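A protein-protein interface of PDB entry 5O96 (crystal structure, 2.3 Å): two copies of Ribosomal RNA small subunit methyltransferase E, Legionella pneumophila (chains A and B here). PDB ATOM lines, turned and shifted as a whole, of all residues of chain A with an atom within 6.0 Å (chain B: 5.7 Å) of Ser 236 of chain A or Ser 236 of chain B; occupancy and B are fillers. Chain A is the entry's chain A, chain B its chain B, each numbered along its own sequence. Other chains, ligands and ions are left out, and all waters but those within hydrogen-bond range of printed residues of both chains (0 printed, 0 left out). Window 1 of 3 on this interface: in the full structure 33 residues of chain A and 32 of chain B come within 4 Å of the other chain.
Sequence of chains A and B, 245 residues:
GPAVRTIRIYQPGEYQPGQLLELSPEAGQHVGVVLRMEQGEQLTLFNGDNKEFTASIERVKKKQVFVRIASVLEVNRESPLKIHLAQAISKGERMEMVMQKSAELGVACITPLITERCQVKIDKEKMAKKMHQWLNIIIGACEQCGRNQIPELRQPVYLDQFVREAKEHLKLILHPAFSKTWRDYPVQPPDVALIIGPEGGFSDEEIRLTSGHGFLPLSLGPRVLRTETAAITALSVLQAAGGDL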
ATOM      1  N   LEU A 105      -1.247  -3.995 -10.362  1.00  0.00           N
ATOM      2  CA  LEU A 105      -1.367  -5.085  -9.414  1.00  0.00           C
ATOM      3  C   LEU A 105      -2.669  -5.854  -9.587  1.00  0.00           C
ATOM      4  O   LEU A 105      -3.120  -6.507  -8.654  1.00  0.00           O
ATOM      5  CB  LEU A 105      -1.197  -4.568  -7.985  1.00  0.00           C
ATOM      6  CG  LEU A 105       0.243  -4.858  -7.563  1.00  0.00           C
ATOM      7  CD1 LEU A 105       1.186  -3.936  -8.294  1.00  0.00           C
ATOM      8  CD2 LEU A 105       0.368  -4.659  -6.146  1.00  0.00           C
ATOM      9  N   ALA A 231      -2.285   1.374  -0.559  1.00  0.00           N
ATOM     10  CA  ALA A 231      -3.007   0.714  -1.637  1.00  0.00           C
ATOM     11  C   ALA A 231      -2.166  -0.384  -2.280  1.00  0.00           C
ATOM     12  O   ALA A 231      -2.625  -1.517  -2.448  1.00  0.00           O
ATOM     13  CB  ALA A 231      -3.426   1.737  -2.688  1.00  0.00           C
ATOM     14  N   ILE A 232      -0.923  -0.063  -2.646  1.00  0.00           N
ATOM     15  CA  ILE A 232      -0.134  -0.997  -3.445  1.00  0.00           C
ATOM     16  C   ILE A 232       0.327  -2.161  -2.604  1.00  0.00           C
ATOM     17  O   ILE A 232       0.252  -3.322  -3.029  1.00  0.00           O
ATOM     18  CB  ILE A 232       1.048  -0.272  -4.080  1.00  0.00           C
ATOM     19  CG1 ILE A 232       0.526   0.957  -4.781  1.00  0.00           C
ATOM     20  CG2 ILE A 232       1.752  -1.157  -5.083  1.00  0.00           C
ATOM     21  CD1 ILE A 232       1.634   1.686  -5.310  1.00  0.00           C
ATOM     22  N   THR A 233       0.777  -1.871  -1.387  1.00  0.00           N
ATOM     23  CA  THR A 233       1.078  -2.918  -0.410  1.00  0.00           C
ATOM     24  C   THR A 233      -0.121  -3.839  -0.182  1.00  0.00           C
ATOM     25  O   THR A 233       0.007  -5.062  -0.213  1.00  0.00           O
ATOM     26  CB  THR A 233       1.513  -2.253   0.889  1.00  0.00           C
ATOM     27  OG1 THR A 233       2.722  -1.526   0.636  1.00  0.00           O
ATOM     28  CG2 THR A 233       1.738  -3.277   1.975  1.00  0.00           C
ATOM     29  N   ALA A 234      -1.307  -3.261   0.038  1.00  0.00           N
ATOM     30  CA  ALA A 234      -2.471  -4.091   0.344  1.00  0.00           C
ATOM     31  C   ALA A 234      -2.813  -4.994  -0.831  1.00  0.00           C
ATOM     32  O   ALA A 234      -3.098  -6.184  -0.657  1.00  0.00           O
ATOM     33  CB  ALA A 234      -3.669  -3.206   0.724  1.00  0.00           C
ATOM     34  N   LEU A 235      -2.771  -4.443  -2.036  1.00  0.00           N
ATOM     35  CA  LEU A 235      -3.014  -5.248  -3.225  1.00  0.00           C
ATOM     36  C   LEU A 235      -1.931  -6.313  -3.411  1.00  0.00           C
ATOM     37  O   LEU A 235      -2.242  -7.469  -3.730  1.00  0.00           O
ATOM     38  CB  LEU A 235      -3.117  -4.335  -4.448  1.00  0.00           C
ATOM     39  CG  LEU A 235      -4.386  -3.467  -4.458  1.00  0.00           C
ATOM     40  CD1 LEU A 235      -4.467  -2.632  -5.712  1.00  0.00           C
ATOM     41  CD2 LEU A 235      -5.619  -4.334  -4.349  1.00  0.00           C
ATOM     42  N   SER A 236      -0.663  -5.955  -3.173  1.00  0.00           N
ATOM     43  CA  SER A 236       0.421  -6.926  -3.264  1.00  0.00           C
ATOM     44  C   SER A 236       0.192  -8.113  -2.334  1.00  0.00           C
ATOM     45  O   SER A 236       0.293  -9.275  -2.754  1.00  0.00           O
ATOM     46  CB  SER A 236       1.759  -6.247  -2.951  1.00  0.00           C
ATOM     47  OG  SER A 236       2.083  -5.263  -3.927  1.00  0.00           O
ATOM     48  N   VAL A 237      -0.095  -7.829  -1.065  1.00  0.00           N
ATOM     49  CA  VAL A 237      -0.315  -8.857  -0.044  1.00  0.00           C
ATOM     50  C   VAL A 237      -1.561  -9.698  -0.350  1.00  0.00           C
ATOM     51  O   VAL A 237      -1.583 -10.917  -0.118  1.00  0.00           O
ATOM     52  CB  VAL A 237      -0.412  -8.181   1.341  1.00  0.00           C
ATOM     53  CG1 VAL A 237      -0.937  -9.128   2.393  1.00  0.00           C
ATOM     54  CG2 VAL A 237       0.945  -7.634   1.730  1.00  0.00           C
ATOM     55  N   LEU A 238      -2.625  -9.075  -0.852  1.00  0.00           N
ATOM     56  CA  LEU A 238      -3.822  -9.876  -1.104  1.00  0.00           C
ATOM     57  C   LEU A 238      -3.646 -10.755  -2.343  1.00  0.00           C
ATOM     58  O   LEU A 238      -4.106 -11.896  -2.362  1.00  0.00           O
ATOM     59  CB  LEU A 238      -5.055  -8.980  -1.249  1.00  0.00           C
ATOM     60  CG  LEU A 238      -5.451  -8.142  -0.020  1.00  0.00           C
ATOM     61  CD1 LEU A 238      -6.572  -7.121  -0.385  1.00  0.00           C
ATOM     62  CD2 LEU A 238      -5.867  -9.039   1.142  1.00  0.00           C
ATOM     63  N   GLN A 239      -2.980 -10.245  -3.382  1.00  0.00           N
ATOM     64  CA  GLN A 239      -2.713 -11.076  -4.547  1.00  0.00           C
ATOM     65  C   GLN A 239      -1.742 -12.195  -4.221  1.00  0.00           C
ATOM     66  O   GLN A 239      -1.868 -13.301  -4.762  1.00  0.00           O
ATOM     67  CB  GLN A 239      -2.185 -10.230  -5.698  1.00  0.00           C
ATOM     68  CG  GLN A 239      -3.211  -9.234  -6.217  1.00  0.00           C
ATOM     69  CD  GLN A 239      -4.359  -9.912  -6.937  1.00  0.00           C
ATOM     70  OE1 GLN A 239      -4.362 -11.127  -7.126  1.00  0.00           O
ATOM     71  NE2 GLN A 239      -5.334  -9.132  -7.342  1.00  0.00           N
ATOM     72  N   ALA A 240      -0.780 -11.934  -3.347  1.00  0.00           N
ATOM     73  CA  ALA A 240       0.173 -12.965  -2.969  1.00  0.00           C
ATOM     74  C   ALA A 240      -0.457 -14.030  -2.093  1.00  0.00           C
ATOM     75  O   ALA A 240       0.074 -15.141  -2.002  1.00  0.00           O
ATOM     76  CB  ALA A 240       1.361 -12.337  -2.223  1.00  0.00           C
ATOM     77  N   ALA A 241      -1.544 -13.694  -1.413  1.00  0.00           N
ATOM     78  CA  ALA A 241      -2.212 -14.608  -0.501  1.00  0.00           C
ATOM     79  C   ALA A 241      -3.194 -15.504  -1.245  1.00  0.00           C
ATOM     80  O   ALA A 241      -3.147 -16.731  -1.115  1.00  0.00           O
ATOM     81  CB  ALA A 241      -2.942 -13.807   0.583  1.00  0.00           C
ATOM     82  N   LEU A 245      -0.064 -13.977  -7.372  1.00  0.00           N
ATOM     83  CA  LEU A 245       1.298 -13.656  -6.986  1.00  0.00           C
ATOM     84  C   LEU A 245       1.930 -14.755  -6.150  1.00  0.00           C
ATOM     85  O   LEU A 245       1.265 -15.549  -5.490  1.00  0.00           O
ATOM     86  CB  LEU A 245       1.336 -12.342  -6.206  1.00  0.00           C
ATOM     87  CG  LEU A 245       1.771 -11.166  -7.072  1.00  0.00           C
ATOM     88  CD1 LEU A 245       0.765 -10.891  -8.159  1.00  0.00           C
ATOM     89  CD2 LEU A 245       2.049  -9.927  -6.250  1.00  0.00           C
ATOM     90  OXT LEU A 245       3.154 -14.866  -6.101  1.00  0.00           O
ATOM     91  N   LEU B 105       8.493   0.241   4.109  1.00  0.00           N
ATOM     92  CA  LEU B 105       8.237  -1.193   4.162  1.00  0.00           C
ATOM     93  C   LEU B 105       9.258  -1.973   4.992  1.00  0.00           C
ATOM     94  O   LEU B 105       9.263  -3.212   4.946  1.00  0.00           O
ATOM     95  CB  LEU B 105       8.161  -1.760   2.736  1.00  0.00           C
ATOM     96  CG  LEU B 105       6.834  -1.346   2.102  1.00  0.00           C
ATOM     97  CD1 LEU B 105       6.883  -1.418   0.585  1.00  0.00           C
ATOM     98  CD2 LEU B 105       5.718  -2.221   2.650  1.00  0.00           C
ATOM     99  N   ALA B 231       9.709  -3.167  -6.533  1.00  0.00           N
ATOM    100  CA  ALA B 231      10.294  -3.044  -5.204  1.00  0.00           C
ATOM    101  C   ALA B 231       9.214  -2.969  -4.136  1.00  0.00           C
ATOM    102  O   ALA B 231       9.337  -3.597  -3.072  1.00  0.00           O
ATOM    103  CB  ALA B 231      11.203  -1.821  -5.127  1.00  0.00           C
ATOM    104  N   ILE B 232       8.169  -2.174  -4.375  1.00  0.00           N
ATOM    105  CA  ILE B 232       7.085  -2.079  -3.390  1.00  0.00           C
ATOM    106  C   ILE B 232       6.423  -3.434  -3.195  1.00  0.00           C
ATOM    107  O   ILE B 232       6.248  -3.908  -2.066  1.00  0.00           O
ATOM    108  CB  ILE B 232       6.039  -1.035  -3.806  1.00  0.00           C
ATOM    109  CG1 ILE B 232       6.654   0.360  -3.921  1.00  0.00           C
ATOM    110  CG2 ILE B 232       4.910  -1.022  -2.797  1.00  0.00           C
ATOM    111  CD1 ILE B 232       5.718   1.364  -4.635  1.00  0.00           C
ATOM    112  N   THR B 233       6.018  -4.065  -4.295  1.00  0.00           N
ATOM    113  CA  THR B 233       5.333  -5.355  -4.206  1.00  0.00           C
ATOM    114  C   THR B 233       6.229  -6.415  -3.568  1.00  0.00           C
ATOM    115  O   THR B 233       5.792  -7.138  -2.663  1.00  0.00           O
ATOM    116  CB  THR B 233       4.876  -5.774  -5.604  1.00  0.00           C
ATOM    117  OG1 THR B 233       4.054  -4.735  -6.170  1.00  0.00           O
ATOM    118  CG2 THR B 233       4.115  -7.082  -5.570  1.00  0.00           C
ATOM    119  N   ALA B 234       7.503  -6.489  -3.983  1.00  0.00           N
ATOM    120  CA  ALA B 234       8.370  -7.561  -3.488  1.00  0.00           C
ATOM    121  C   ALA B 234       8.588  -7.452  -1.993  1.00  0.00           C
ATOM    122  O   ALA B 234       8.608  -8.462  -1.285  1.00  0.00           O
ATOM    123  CB  ALA B 234       9.732  -7.538  -4.200  1.00  0.00           C
ATOM    124  N   LEU B 235       8.794  -6.230  -1.500  1.00  0.00           N
ATOM    125  CA  LEU B 235       8.970  -6.032  -0.070  1.00  0.00           C
ATOM    126  C   LEU B 235       7.675  -6.302   0.689  1.00  0.00           C
ATOM    127  O   LEU B 235       7.693  -6.910   1.763  1.00  0.00           O
ATOM    128  CB  LEU B 235       9.467  -4.609   0.200  1.00  0.00           C
ATOM    129  CG  LEU B 235      10.895  -4.252  -0.277  1.00  0.00           C
ATOM    130  CD1 LEU B 235      11.422  -3.090   0.518  1.00  0.00           C
ATOM    131  CD2 LEU B 235      11.833  -5.385  -0.158  1.00  0.00           C
ATOM    132  N   SER B 236       6.541  -5.845   0.157  1.00  0.00           N
ATOM    133  CA  SER B 236       5.264  -6.159   0.786  1.00  0.00           C
ATOM    134  C   SER B 236       5.091  -7.665   0.906  1.00  0.00           C
ATOM    135  O   SER B 236       4.785  -8.181   1.988  1.00  0.00           O
ATOM    136  CB  SER B 236       4.106  -5.543  -0.016  1.00  0.00           C
ATOM    137  OG  SER B 236       4.242  -4.132  -0.091  1.00  0.00           O
ATOM    138  N   VAL B 237       5.315  -8.392  -0.193  1.00  0.00           N
ATOM    139  CA  VAL B 237       5.108  -9.839  -0.167  1.00  0.00           C
ATOM    140  C   VAL B 237       6.076 -10.511   0.800  1.00  0.00           C
ATOM    141  O   VAL B 237       5.670 -11.358   1.609  1.00  0.00           O
ATOM    142  CB  VAL B 237       5.209 -10.419  -1.581  1.00  0.00           C
ATOM    143  CG1 VAL B 237       5.282 -11.930  -1.525  1.00  0.00           C
ATOM    144  CG2 VAL B 237       4.027  -9.954  -2.424  1.00  0.00           C
ATOM    145  N   LEU B 238       7.354 -10.109   0.776  1.00  0.00           N
ATOM    146  CA  LEU B 238       8.340 -10.734   1.662  1.00  0.00           C
ATOM    147  C   LEU B 238       8.080 -10.404   3.134  1.00  0.00           C
ATOM    148  O   LEU B 238       8.280 -11.256   4.010  1.00  0.00           O
ATOM    149  CB  LEU B 238       9.773 -10.318   1.285  1.00  0.00           C
ATOM    150  CG  LEU B 238      10.387 -10.752  -0.051  1.00  0.00           C
ATOM    151  CD1 LEU B 238      11.786 -10.191  -0.214  1.00  0.00           C
ATOM    152  CD2 LEU B 238      10.411 -12.264  -0.196  1.00  0.00           C
ATOM    153  N   GLN B 239       7.633  -9.182   3.444  1.00  0.00           N
ATOM    154  CA  GLN B 239       7.302  -8.915   4.838  1.00  0.00           C
ATOM    155  C   GLN B 239       6.030  -9.661   5.244  1.00  0.00           C
ATOM    156  O   GLN B 239       5.937 -10.172   6.363  1.00  0.00           O
ATOM    157  CB  GLN B 239       7.170  -7.408   5.093  1.00  0.00           C
ATOM    158  CG  GLN B 239       8.438  -6.616   4.766  1.00  0.00           C
ATOM    159  CD  GLN B 239       9.493  -6.692   5.851  1.00  0.00           C
ATOM    160  OE1 GLN B 239       9.521  -7.620   6.646  1.00  0.00           O
ATOM    161  NE2 GLN B 239      10.361  -5.694   5.897  1.00  0.00           N
ATOM    162  N   ALA B 240       5.061  -9.782   4.330  1.00  0.00           N
ATOM    163  CA  ALA B 240       3.843 -10.523   4.630  1.00  0.00           C
ATOM    164  C   ALA B 240       4.130 -11.988   4.876  1.00  0.00           C
ATOM    165  O   ALA B 240       3.469 -12.612   5.709  1.00  0.00           O
ATOM    166  CB  ALA B 240       2.843 -10.375   3.488  1.00  0.00           C
ATOM    167  N   ALA B 241       5.114 -12.549   4.167  1.00  0.00           N
ATOM    168  CA  ALA B 241       5.407 -13.979   4.245  1.00  0.00           C
ATOM    169  C   ALA B 241       6.235 -14.316   5.469  1.00  0.00           C
ATOM    170  O   ALA B 241       5.931 -15.274   6.187  1.00  0.00           O
ATOM    171  CB  ALA B 241       6.146 -14.422   2.984  1.00  0.00           C
ATOM    172  N   LEU B 245       4.287  -8.074   8.386  1.00  0.00           N
ATOM    173  CA  LEU B 245       3.077  -7.643   7.690  1.00  0.00           C
ATOM    174  C   LEU B 245       1.987  -8.695   7.799  1.00  0.00           C
ATOM    175  O   LEU B 245       2.277  -9.892   7.746  1.00  0.00           O
ATOM    176  CB  LEU B 245       3.343  -7.348   6.218  1.00  0.00           C
ATOM    177  CG  LEU B 245       3.311  -5.857   5.907  1.00  0.00           C
ATOM    178  CD1 LEU B 245       4.558  -5.153   6.504  1.00  0.00           C
ATOM    179  CD2 LEU B 245       3.172  -5.606   4.426  1.00  0.00           C
ATOM    180  OXT LEU B 245       0.798  -8.363   7.939  1.00  0.00           O
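Leu 105 of chain A touches Thr 233 of chain B, and with the chains exchanged Thr 233 of chain A touches Leu 105 of chain B. Ile 232 of chain A touches its own counterpart, Ile 232 of chain B. Thr 233 of chain A touches Leu 245 of chain B, and with the chains exchanged Leu 245 of chain A touches Thr 233 of chain B. Ser 236 of chain A touches Val 237 of chain B, and with the chains exchanged Val 237 of chain A touches Ser 236 of chain B.
Of chain B, only Thr 233 (3.0 Å), Ser 236 (3.8 Å) and Val 237 (3.8 Å) come within 4 Å of Ser 236 of chain A. Of the printed residues of chain A, Ser 236 of chain B touches Thr 233 (3.1 Å), Ser 236 (3.8 Å) and Val 237 (3.9 Å). Of the printed residues of chain B, Leu 105 of chain A touches Thr 233. Of the printed residues of chain B, Val 237 of chain A touches Ser 236 (3.9 Å) and Ala 240 (3.8 Å). Of the printed residues of chain B, Leu 245 of chain A touches Thr 233. Printed residues of chain B within 4 Å of Ala 240 of chain A: Val 237 (3.6 Å). Of the printed residues of chain A, Val 237 of chain B touches Ser 236 and Ala 240. Leu 235 of chain B touches none of the printed residues of chain A. Leu 238 of chain A touches none of the printed residues of chain B. The nearest printed residue of chain B that does not touch Leu 245 of chain A is Val 237 of chain B (4.3 Å).
Among the printed residues, merely in contact across the chains: Leu 105 of chain A with Thr 233 of chain B (3.7 Å), Ile 232 of chain A with Ile 232 of chain B (3.9 Å), Thr 233 of chain A with Leu 105 of chain B (3.7 Å), Thr 233 of chain A with Leu 245 of chain B (3.7 Å), Ser 236 of chain A with Ser 236 of chain B (3.8 Å), Ser 236 of chain A with Val 237 of chain B (3.8 Å), Val 237 of chain A with Ser 236 of chain B (3.9 Å), Val 237 of chain A with Ala 240 of chain B (3.8 Å), Ala 240 of chain A with Val 237 of chain B (3.6 Å) and Leu 245 of chain A with Thr 233 of chain B (3.6 Å).
Of the 13 printed residues of chain A, 7 touch a printed residue of chain B. Hydrophobic or aromatic side chains of chain A that line the printed part of chain B: Leu 105, Ile 232, Val 237, Ala 240 and Leu 245. Hydrophobic or aromatic side chains of chain B that line the printed part of chain A: Leu 105, Ile 232, Val 237, Ala 240 and Leu 245. Among the printed residues, no Asp or Glu carboxylate lies within 4 Å of a Lys or Arg side-chain nitrogen of the other chain.
The backbone carbonyl oxygen (O) of Ile 232 of chain A lies within hydrogen-bond range of the side-chain hydroxyl (OG) of Ser 236 of chain A. O of Gln 239 of chain A lies within hydrogen-bond range of N of Leu 245 of chain A, at 3.2 Å. NE2 of Gln 239 of chain B sits at hydrogen-bond distance from O of Leu 105 of chain B (2.9 Å). The backbone carbonyl oxygen (O) of Ile 232 of chain B sits at hydrogen-bond distance from the side-chain hydroxyl (OG) of Ser 236 of chain B. The backbone NH (N) of Leu 245 of chain B is in hydrogen-bond range of the backbone carbonyl oxygen (O) of Gln 239 of chain B (3.3 Å).
OG1 of Thr 233 of chain A sits at hydrogen-bond distance from OG of Ser 236 of chain B, 3.1 Å away. OG1 of Thr 233 of chain B lies within hydrogen-bond range of OG of Ser 236 of chain A, at 3.0 Å.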
